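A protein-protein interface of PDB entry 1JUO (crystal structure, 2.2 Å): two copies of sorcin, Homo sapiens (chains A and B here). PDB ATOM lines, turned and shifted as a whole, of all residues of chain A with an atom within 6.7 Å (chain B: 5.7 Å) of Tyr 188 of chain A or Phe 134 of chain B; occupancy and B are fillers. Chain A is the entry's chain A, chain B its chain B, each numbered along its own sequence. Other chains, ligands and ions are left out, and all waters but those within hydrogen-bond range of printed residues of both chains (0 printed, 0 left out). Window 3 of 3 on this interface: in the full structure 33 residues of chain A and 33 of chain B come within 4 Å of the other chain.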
ATOM      1  N   PHE A 186     -17.429   0.164  30.897  1.00  0.00           N
ATOM      2  CA  PHE A 186     -16.005  -0.091  30.810  1.00  0.00           C
ATOM      3  C   PHE A 186     -15.188   1.122  30.422  1.00  0.00           C
ATOM      4  O   PHE A 186     -15.432   1.721  29.376  1.00  0.00           O
ATOM      5  CB  PHE A 186     -15.753  -1.174  29.770  1.00  0.00           C
ATOM      6  CG  PHE A 186     -15.562  -2.541  30.339  1.00  0.00           C
ATOM      7  CD1 PHE A 186     -14.399  -2.861  31.034  1.00  0.00           C
ATOM      8  CD2 PHE A 186     -16.522  -3.529  30.142  1.00  0.00           C
ATOM      9  CE1 PHE A 186     -14.192  -4.144  31.519  1.00  0.00           C
ATOM     10  CE2 PHE A 186     -16.321  -4.823  30.628  1.00  0.00           C
ATOM     11  CZ  PHE A 186     -15.154  -5.128  31.316  1.00  0.00           C
ATOM     12  N   PRO A 187     -14.233   1.530  31.275  1.00  0.00           N
ATOM     13  CA  PRO A 187     -13.415   2.687  30.908  1.00  0.00           C
ATOM     14  C   PRO A 187     -12.399   2.073  29.957  1.00  0.00           C
ATOM     15  O   PRO A 187     -12.043   0.909  30.118  1.00  0.00           O
ATOM     16  CB  PRO A 187     -12.787   3.107  32.231  1.00  0.00           C
ATOM     17  CG  PRO A 187     -13.803   2.664  33.238  1.00  0.00           C
ATOM     18  CD  PRO A 187     -14.166   1.299  32.729  1.00  0.00           C
ATOM     19  N   TYR A 188     -11.935   2.829  28.972  1.00  0.00           N
ATOM     20  CA  TYR A 188     -10.987   2.286  28.015  1.00  0.00           C
ATOM     21  C   TYR A 188      -9.772   1.547  28.595  1.00  0.00           C
ATOM     22  O   TYR A 188      -9.500   0.412  28.203  1.00  0.00           O
ATOM     23  CB  TYR A 188     -10.517   3.389  27.065  1.00  0.00           C
ATOM     24  CG  TYR A 188      -9.527   2.899  26.037  1.00  0.00           C
ATOM     25  CD1 TYR A 188      -8.158   3.097  26.203  1.00  0.00           C
ATOM     26  CD2 TYR A 188      -9.960   2.193  24.916  1.00  0.00           C
ATOM     27  CE1 TYR A 188      -7.241   2.608  25.277  1.00  0.00           C
ATOM     28  CE2 TYR A 188      -9.056   1.697  23.986  1.00  0.00           C
ATOM     29  CZ  TYR A 188      -7.698   1.910  24.168  1.00  0.00           C
ATOM     30  OH  TYR A 188      -6.807   1.457  23.216  1.00  0.00           O
ATOM     31  N   ASP A 189      -9.041   2.155  29.522  1.00  0.00           N
ATOM     32  CA  ASP A 189      -7.862   1.479  30.061  1.00  0.00           C
ATOM     33  C   ASP A 189      -8.204   0.128  30.681  1.00  0.00           C
ATOM     34  O   ASP A 189      -7.481  -0.853  30.491  1.00  0.00           O
ATOM     35  CB  ASP A 189      -7.149   2.349  31.100  1.00  0.00           C
ATOM     36  CG  ASP A 189      -5.713   1.884  31.367  1.00  0.00           C
ATOM     37  OD1 ASP A 189      -4.834   2.117  30.509  1.00  0.00           O
ATOM     38  OD2 ASP A 189      -5.457   1.274  32.429  1.00  0.00           O
ATOM     39  N   ASP A 190      -9.316   0.074  31.410  1.00  0.00           N
ATOM     40  CA  ASP A 190      -9.751  -1.160  32.066  1.00  0.00           C
ATOM     41  C   ASP A 190     -10.135  -2.215  31.033  1.00  0.00           C
ATOM     42  O   ASP A 190      -9.741  -3.375  31.133  1.00  0.00           O
ATOM     43  CB  ASP A 190     -10.934  -0.860  32.991  1.00  0.00           C
ATOM     44  CG  ASP A 190     -11.377  -2.068  33.782  1.00  0.00           C
ATOM     45  OD1 ASP A 190     -10.507  -2.762  34.339  1.00  0.00           O
ATOM     46  OD2 ASP A 190     -12.600  -2.318  33.853  1.00  0.00           O
ATOM     47  N   PHE A 191     -10.903  -1.801  30.033  1.00  0.00           N
ATOM     48  CA  PHE A 191     -11.325  -2.701  28.970  1.00  0.00           C
ATOM     49  C   PHE A 191     -10.118  -3.315  28.273  1.00  0.00           C
ATOM     50  O   PHE A 191     -10.091  -4.509  27.982  1.00  0.00           O
ATOM     51  CB  PHE A 191     -12.182  -1.933  27.963  1.00  0.00           C
ATOM     52  CG  PHE A 191     -12.496  -2.700  26.706  1.00  0.00           C
ATOM     53  CD1 PHE A 191     -11.680  -2.584  25.584  1.00  0.00           C
ATOM     54  CD2 PHE A 191     -13.639  -3.489  26.625  1.00  0.00           C
ATOM     55  CE1 PHE A 191     -12.000  -3.236  24.400  1.00  0.00           C
ATOM     56  CE2 PHE A 191     -13.963  -4.140  25.454  1.00  0.00           C
ATOM     57  CZ  PHE A 191     -13.146  -4.013  24.334  1.00  0.00           C
ATOM     58  N   ILE A 192      -9.110  -2.497  28.009  1.00  0.00           N
ATOM     59  CA  ILE A 192      -7.919  -2.993  27.337  1.00  0.00           C
ATOM     60  C   ILE A 192      -7.113  -3.995  28.146  1.00  0.00           C
ATOM     61  O   ILE A 192      -6.775  -5.060  27.646  1.00  0.00           O
ATOM     62  CB  ILE A 192      -6.975  -1.837  26.922  1.00  0.00           C
ATOM     63  CG1 ILE A 192      -7.564  -1.082  25.735  1.00  0.00           C
ATOM     64  CG2 ILE A 192      -5.613  -2.393  26.519  1.00  0.00           C
ATOM     65  CD1 ILE A 192      -7.751  -1.946  24.507  1.00  0.00           C
ATOM     66  N   GLN A 193      -6.794  -3.657  29.391  1.00  0.00           N
ATOM     67  CA  GLN A 193      -5.989  -4.554  30.212  1.00  0.00           C
ATOM     68  C   GLN A 193      -6.737  -5.840  30.504  1.00  0.00           C
ATOM     69  O   GLN A 193      -6.144  -6.891  30.732  1.00  0.00           O
ATOM     70  CB  GLN A 193      -5.579  -3.862  31.523  1.00  0.00           C
ATOM     71  CG  GLN A 193      -6.699  -3.616  32.514  1.00  0.00           C
ATOM     72  CD  GLN A 193      -7.050  -4.852  33.310  1.00  0.00           C
ATOM     73  OE1 GLN A 193      -8.086  -4.898  33.972  1.00  0.00           O
ATOM     74  NE2 GLN A 193      -6.182  -5.863  33.260  1.00  0.00           N
ATOM     75  N   GLN B 126       6.027  -0.244  26.344  1.00  0.00           N
ATOM     76  CA  GLN B 126       5.150   0.893  26.587  1.00  0.00           C
ATOM     77  C   GLN B 126       5.632   2.097  25.793  1.00  0.00           C
ATOM     78  O   GLN B 126       4.855   2.993  25.474  1.00  0.00           O
ATOM     79  CB  GLN B 126       5.100   1.244  28.078  1.00  0.00           C
ATOM     80  CG  GLN B 126       4.133   2.388  28.409  1.00  0.00           C
ATOM     81  CD  GLN B 126       4.020   2.654  29.906  1.00  0.00           C
ATOM     82  OE1 GLN B 126       5.026   2.839  30.597  1.00  0.00           O
ATOM     83  NE2 GLN B 126       2.792   2.681  30.411  1.00  0.00           N
ATOM     84  N   LEU B 129       4.500   1.428  22.194  1.00  0.00           N
ATOM     85  CA  LEU B 129       3.053   1.620  22.206  1.00  0.00           C
ATOM     86  C   LEU B 129       2.651   3.077  22.354  1.00  0.00           C
ATOM     87  O   LEU B 129       1.673   3.517  21.750  1.00  0.00           O
ATOM     88  CB  LEU B 129       2.420   0.777  23.320  1.00  0.00           C
ATOM     89  CG  LEU B 129       1.827  -0.583  22.918  1.00  0.00           C
ATOM     90  CD1 LEU B 129       2.785  -1.333  22.023  1.00  0.00           C
ATOM     91  CD2 LEU B 129       1.509  -1.399  24.170  1.00  0.00           C
ATOM     92  N   THR B 130       3.403   3.832  23.148  1.00  0.00           N
ATOM     93  CA  THR B 130       3.100   5.246  23.353  1.00  0.00           C
ATOM     94  C   THR B 130       3.446   6.094  22.122  1.00  0.00           C
ATOM     95  O   THR B 130       2.649   6.935  21.701  1.00  0.00           O
ATOM     96  CB  THR B 130       3.854   5.819  24.578  1.00  0.00           C
ATOM     97  OG1 THR B 130       5.199   5.327  24.584  1.00  0.00           O
ATOM     98  CG2 THR B 130       3.163   5.431  25.871  1.00  0.00           C
ATOM     99  N   THR B 131       4.632   5.878  21.552  1.00  0.00           N
ATOM    100  CA  THR B 131       5.037   6.630  20.367  1.00  0.00           C
ATOM    101  C   THR B 131       4.073   6.304  19.231  1.00  0.00           C
ATOM    102  O   THR B 131       3.970   7.044  18.254  1.00  0.00           O
ATOM    103  CB  THR B 131       6.470   6.281  19.924  1.00  0.00           C
ATOM    104  OG1 THR B 131       6.540   4.899  19.554  1.00  0.00           O
ATOM    105  CG2 THR B 131       7.451   6.549  21.048  1.00  0.00           C
ATOM    106  N   MET B 132       3.370   5.184  19.371  1.00  0.00           N
ATOM    107  CA  MET B 132       2.387   4.750  18.386  1.00  0.00           C
ATOM    108  C   MET B 132       1.064   5.450  18.664  1.00  0.00           C
ATOM    109  O   MET B 132       0.104   5.291  17.920  1.00  0.00           O
ATOM    110  CB  MET B 132       2.186   3.240  18.471  1.00  0.00           C
ATOM    111  CG  MET B 132       2.672   2.473  17.262  1.00  0.00           C
ATOM    112  SD  MET B 132       2.518   0.698  17.518  1.00  0.00           S
ATOM    113  CE  MET B 132       0.776   0.498  17.290  1.00  0.00           C
ATOM    114  N   GLY B 133       1.017   6.214  19.753  1.00  0.00           N
ATOM    115  CA  GLY B 133      -0.192   6.940  20.095  1.00  0.00           C
ATOM    116  C   GLY B 133      -0.939   6.464  21.330  1.00  0.00           C
ATOM    117  O   GLY B 133      -1.657   7.246  21.958  1.00  0.00           O
ATOM    118  N   PHE B 134      -0.787   5.188  21.682  1.00  0.00           N
ATOM    119  CA  PHE B 134      -1.469   4.627  22.851  1.00  0.00           C
ATOM    120  C   PHE B 134      -0.958   5.210  24.159  1.00  0.00           C
ATOM    121  O   PHE B 134       0.221   5.549  24.291  1.00  0.00           O
ATOM    122  CB  PHE B 134      -1.285   3.112  22.909  1.00  0.00           C
ATOM    123  CG  PHE B 134      -1.966   2.373  21.803  1.00  0.00           C
ATOM    124  CD1 PHE B 134      -3.340   2.172  21.825  1.00  0.00           C
ATOM    125  CD2 PHE B 134      -1.229   1.856  20.744  1.00  0.00           C
ATOM    126  CE1 PHE B 134      -3.969   1.462  20.808  1.00  0.00           C
ATOM    127  CE2 PHE B 134      -1.848   1.148  19.725  1.00  0.00           C
ATOM    128  CZ  PHE B 134      -3.218   0.948  19.757  1.00  0.00           C
ATOM    129  N   ARG B 135      -1.864   5.321  25.122  1.00  0.00           N
ATOM    130  CA  ARG B 135      -1.530   5.823  26.443  1.00  0.00           C
ATOM    131  C   ARG B 135      -2.073   4.835  27.473  1.00  0.00           C
ATOM    132  O   ARG B 135      -2.828   5.198  28.367  1.00  0.00           O
ATOM    133  CB  ARG B 135      -2.128   7.216  26.658  1.00  0.00           C
ATOM    134  CG  ARG B 135      -1.480   8.299  25.803  1.00  0.00           C
ATOM    135  CD  ARG B 135      -0.013   8.510  26.185  1.00  0.00           C
ATOM    136  NE  ARG B 135       0.652   9.496  25.329  1.00  0.00           N
ATOM    137  CZ  ARG B 135       1.195   9.228  24.140  1.00  0.00           C
ATOM    138  NH1 ARG B 135       1.166   7.995  23.644  1.00  0.00           N
ATOM    139  NH2 ARG B 135       1.767  10.201  23.441  1.00  0.00           N
ATOM    140  N   LEU B 136      -1.681   3.574  27.315  1.00  0.00           N
ATOM    141  CA  LEU B 136      -2.091   2.503  28.213  1.00  0.00           C
ATOM    142  C   LEU B 136      -1.386   2.651  29.559  1.00  0.00           C
ATOM    143  O   LEU B 136      -0.272   3.165  29.628  1.00  0.00           O
ATOM    144  CB  LEU B 136      -1.741   1.153  27.597  1.00  0.00           C
ATOM    145  CG  LEU B 136      -2.274   0.953  26.177  1.00  0.00           C
ATOM    146  CD1 LEU B 136      -1.887  -0.432  25.686  1.00  0.00           C
ATOM    147  CD2 LEU B 136      -3.787   1.134  26.158  1.00  0.00           C
ATOM    148  N   LEU B 166      -4.778  -5.006  19.497  1.00  0.00           N
ATOM    149  CA  LEU B 166      -4.942  -3.675  20.053  1.00  0.00           C
ATOM    150  C   LEU B 166      -5.714  -2.821  19.040  1.00  0.00           C
ATOM    151  O   LEU B 166      -6.595  -2.051  19.411  1.00  0.00           O
ATOM    152  CB  LEU B 166      -3.562  -3.081  20.349  1.00  0.00           C
ATOM    153  CG  LEU B 166      -3.297  -2.338  21.664  1.00  0.00           C
ATOM    154  CD1 LEU B 166      -3.908  -3.077  22.831  1.00  0.00           C
ATOM    155  CD2 LEU B 166      -1.792  -2.199  21.861  1.00  0.00           C
ATOM    156  N   ARG B 167      -5.406  -2.972  17.755  1.00  0.00           N
ATOM    157  CA  ARG B 167      -6.104  -2.199  16.726  1.00  0.00           C
ATOM    158  C   ARG B 167      -7.565  -2.604  16.614  1.00  0.00           C
ATOM    159  O   ARG B 167      -8.443  -1.752  16.511  1.00  0.00           O
ATOM    160  CB  ARG B 167      -5.433  -2.361  15.359  1.00  0.00           C
ATOM    161  CG  ARG B 167      -6.275  -1.812  14.193  1.00  0.00           C
ATOM    162  CD  ARG B 167      -5.443  -1.594  12.931  1.00  0.00           C
ATOM    163  NE  ARG B 167      -4.428  -0.568  13.150  1.00  0.00           N
ATOM    164  CZ  ARG B 167      -3.568  -0.148  12.235  1.00  0.00           C
ATOM    165  NH1 ARG B 167      -3.592  -0.665  11.017  1.00  0.00           N
ATOM    166  NH2 ARG B 167      -2.681   0.792  12.539  1.00  0.00           N
ATOM    167  N   LEU B 169      -9.510  -4.218  18.929  1.00  0.00           N
ATOM    168  CA  LEU B 169     -10.213  -3.892  20.163  1.00  0.00           C
ATOM    169  C   LEU B 169     -10.407  -2.399  20.353  1.00  0.00           C
ATOM    170  O   LEU B 169     -11.432  -1.966  20.867  1.00  0.00           O
ATOM    171  CB  LEU B 169      -9.473  -4.487  21.364  1.00  0.00           C
ATOM    172  CG  LEU B 169      -9.557  -6.015  21.400  1.00  0.00           C
ATOM    173  CD1 LEU B 169      -8.470  -6.591  22.294  1.00  0.00           C
ATOM    174  CD2 LEU B 169     -10.948  -6.434  21.873  1.00  0.00           C
ATOM    175  N   THR B 170      -9.436  -1.604  19.927  1.00  0.00           N
ATOM    176  CA  THR B 170      -9.563  -0.164  20.085  1.00  0.00           C
ATOM    177  C   THR B 170     -10.595   0.371  19.105  1.00  0.00           C
ATOM    178  O   THR B 170     -11.323   1.311  19.417  1.00  0.00           O
ATOM    179  CB  THR B 170      -8.217   0.533  19.903  1.00  0.00           C
ATOM    180  OG1 THR B 170      -7.334   0.096  20.943  1.00  0.00           O
ATOM    181  CG2 THR B 170      -8.370   2.049  19.985  1.00  0.00           C
ATOM    182  N   PHE B 173     -13.990  -0.414  20.693  1.00  0.00           N
ATOM    183  CA  PHE B 173     -14.314   0.442  21.827  1.00  0.00           C
ATOM    184  C   PHE B 173     -14.752   1.828  21.343  1.00  0.00           C
ATOM    185  O   PHE B 173     -15.842   2.280  21.657  1.00  0.00           O
ATOM    186  CB  PHE B 173     -13.102   0.575  22.754  1.00  0.00           C
ATOM    187  CG  PHE B 173     -13.379   1.367  23.999  1.00  0.00           C
ATOM    188  CD1 PHE B 173     -13.849   0.738  25.152  1.00  0.00           C
ATOM    189  CD2 PHE B 173     -13.221   2.751  24.008  1.00  0.00           C
ATOM    190  CE1 PHE B 173     -14.165   1.473  26.300  1.00  0.00           C
ATOM    191  CE2 PHE B 173     -13.534   3.500  25.149  1.00  0.00           C
ATOM    192  CZ  PHE B 173     -14.009   2.858  26.298  1.00  0.00           C
ATOM    193  N   GLY B 182     -14.626   8.318  26.938  1.00  0.00           N
ATOM    194  CA  GLY B 182     -13.654   7.262  27.123  1.00  0.00           C
ATOM    195  C   GLY B 182     -14.234   6.089  27.887  1.00  0.00           C
ATOM    196  O   GLY B 182     -13.516   5.170  28.256  1.00  0.00           O
ATOM    197  N   VAL B 183     -15.540   6.120  28.124  1.00  0.00           N
ATOM    198  CA  VAL B 183     -16.216   5.048  28.843  1.00  0.00           C
ATOM    199  C   VAL B 183     -17.333   4.469  27.981  1.00  0.00           C
ATOM    200  O   VAL B 183     -18.153   5.210  27.457  1.00  0.00           O
ATOM    201  CB  VAL B 183     -16.841   5.559  30.150  1.00  0.00           C
ATOM    202  CG1 VAL B 183     -17.450   4.400  30.916  1.00  0.00           C
ATOM    203  CG2 VAL B 183     -15.792   6.270  30.985  1.00  0.00           C
ATOM    204  N   VAL B 184     -17.374   3.147  27.840  1.00  0.00           N
ATOM    205  CA  VAL B 184     -18.409   2.516  27.026  1.00  0.00           C
ATOM    206  C   VAL B 184     -19.366   1.654  27.833  1.00  0.00           C
ATOM    207  O   VAL B 184     -18.954   0.889  28.699  1.00  0.00           O
ATOM    208  CB  VAL B 184     -17.792   1.651  25.905  1.00  0.00           C
ATOM    209  CG1 VAL B 184     -18.880   0.849  25.189  1.00  0.00           C
ATOM    210  CG2 VAL B 184     -17.069   2.543  24.906  1.00  0.00           C
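The backbone carbonyl oxygen (O) of Val 184 of chain B sits at hydrogen-bond distance from the backbone NH (N) of Phe 186 of chain A (2.8 Å). OG1 of Thr 170 of chain B is in hydrogen-bond range of OH of Tyr 188 of chain A. O of Gly 182 of chain B sits at hydrogen-bond distance from N of Tyr 188 of chain A (2.9 Å).
Of the printed residues of chain B, Asp 189 of chain A touches Leu 136 (3.6 Å). Printed residues of chain B within 4 Å of Phe 191 of chain A: Leu 169 and Phe 173. Thr 130 of chain B touches none of the printed residues of chain A. Phe 134 of chain B touches just one residue of chain A: Tyr 188. Of the printed residues of chain A, Phe 173 of chain B touches Phe 186, Tyr 188 and Phe 191. The nearest residue of chain A that does not touch Phe 134 of chain B is Ile 192 of chain A (6.3 Å).
Among the printed residues, pairs that only touch across the chains: Phe 186 of chain A with Phe 173 of chain B (3.3 Å), Tyr 188 of chain A with Phe 173 of chain B (3.4 Å), Phe 186 of chain A with Val 183 of chain B (3.5 Å), Asp 189 of chain A with Leu 136 of chain B (3.6 Å), Pro 187 of chain A with Gly 182 of chain B (3.6 Å), Tyr 188 of chain A with Phe 134 of chain B (3.7 Å), Phe 191 of chain A with Leu 169 of chain B (3.8 Å), Tyr 188 of chain A with Leu 136 of chain B (3.9 Å), Ile 192 of chain A with Leu 136 of chain B (3.99 Å) and Phe 191 of chain A with Phe 173 of chain B (3.99 Å).
No position is printed for both chains. Of the 13 pairs that touch across the chains among the printed residues, none has its exchanged pair printed and touching as well.
The side-chain amide nitrogen (NE2) of Gln 126 of chain B lies within hydrogen-bond range of the backbone carbonyl oxygen (O) of Leu 136 of chain B (3.2 Å). The backbone carbonyl oxygen of Leu 129 of chain B sits at hydrogen-bond distance from the backbone NH of Phe 134 of chain B (3.0 Å). The side-chain hydroxyl (OG1) of Thr 170 of chain B lies within hydrogen-bond range of the backbone carbonyl oxygen (O) of Leu 166 of chain B (2.7 Å).
Of the 17 printed residues of chain B, 8 touch a printed residue of chain A. Of the 8 printed residues of chain A, 6 touch a printed residue of chain B.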
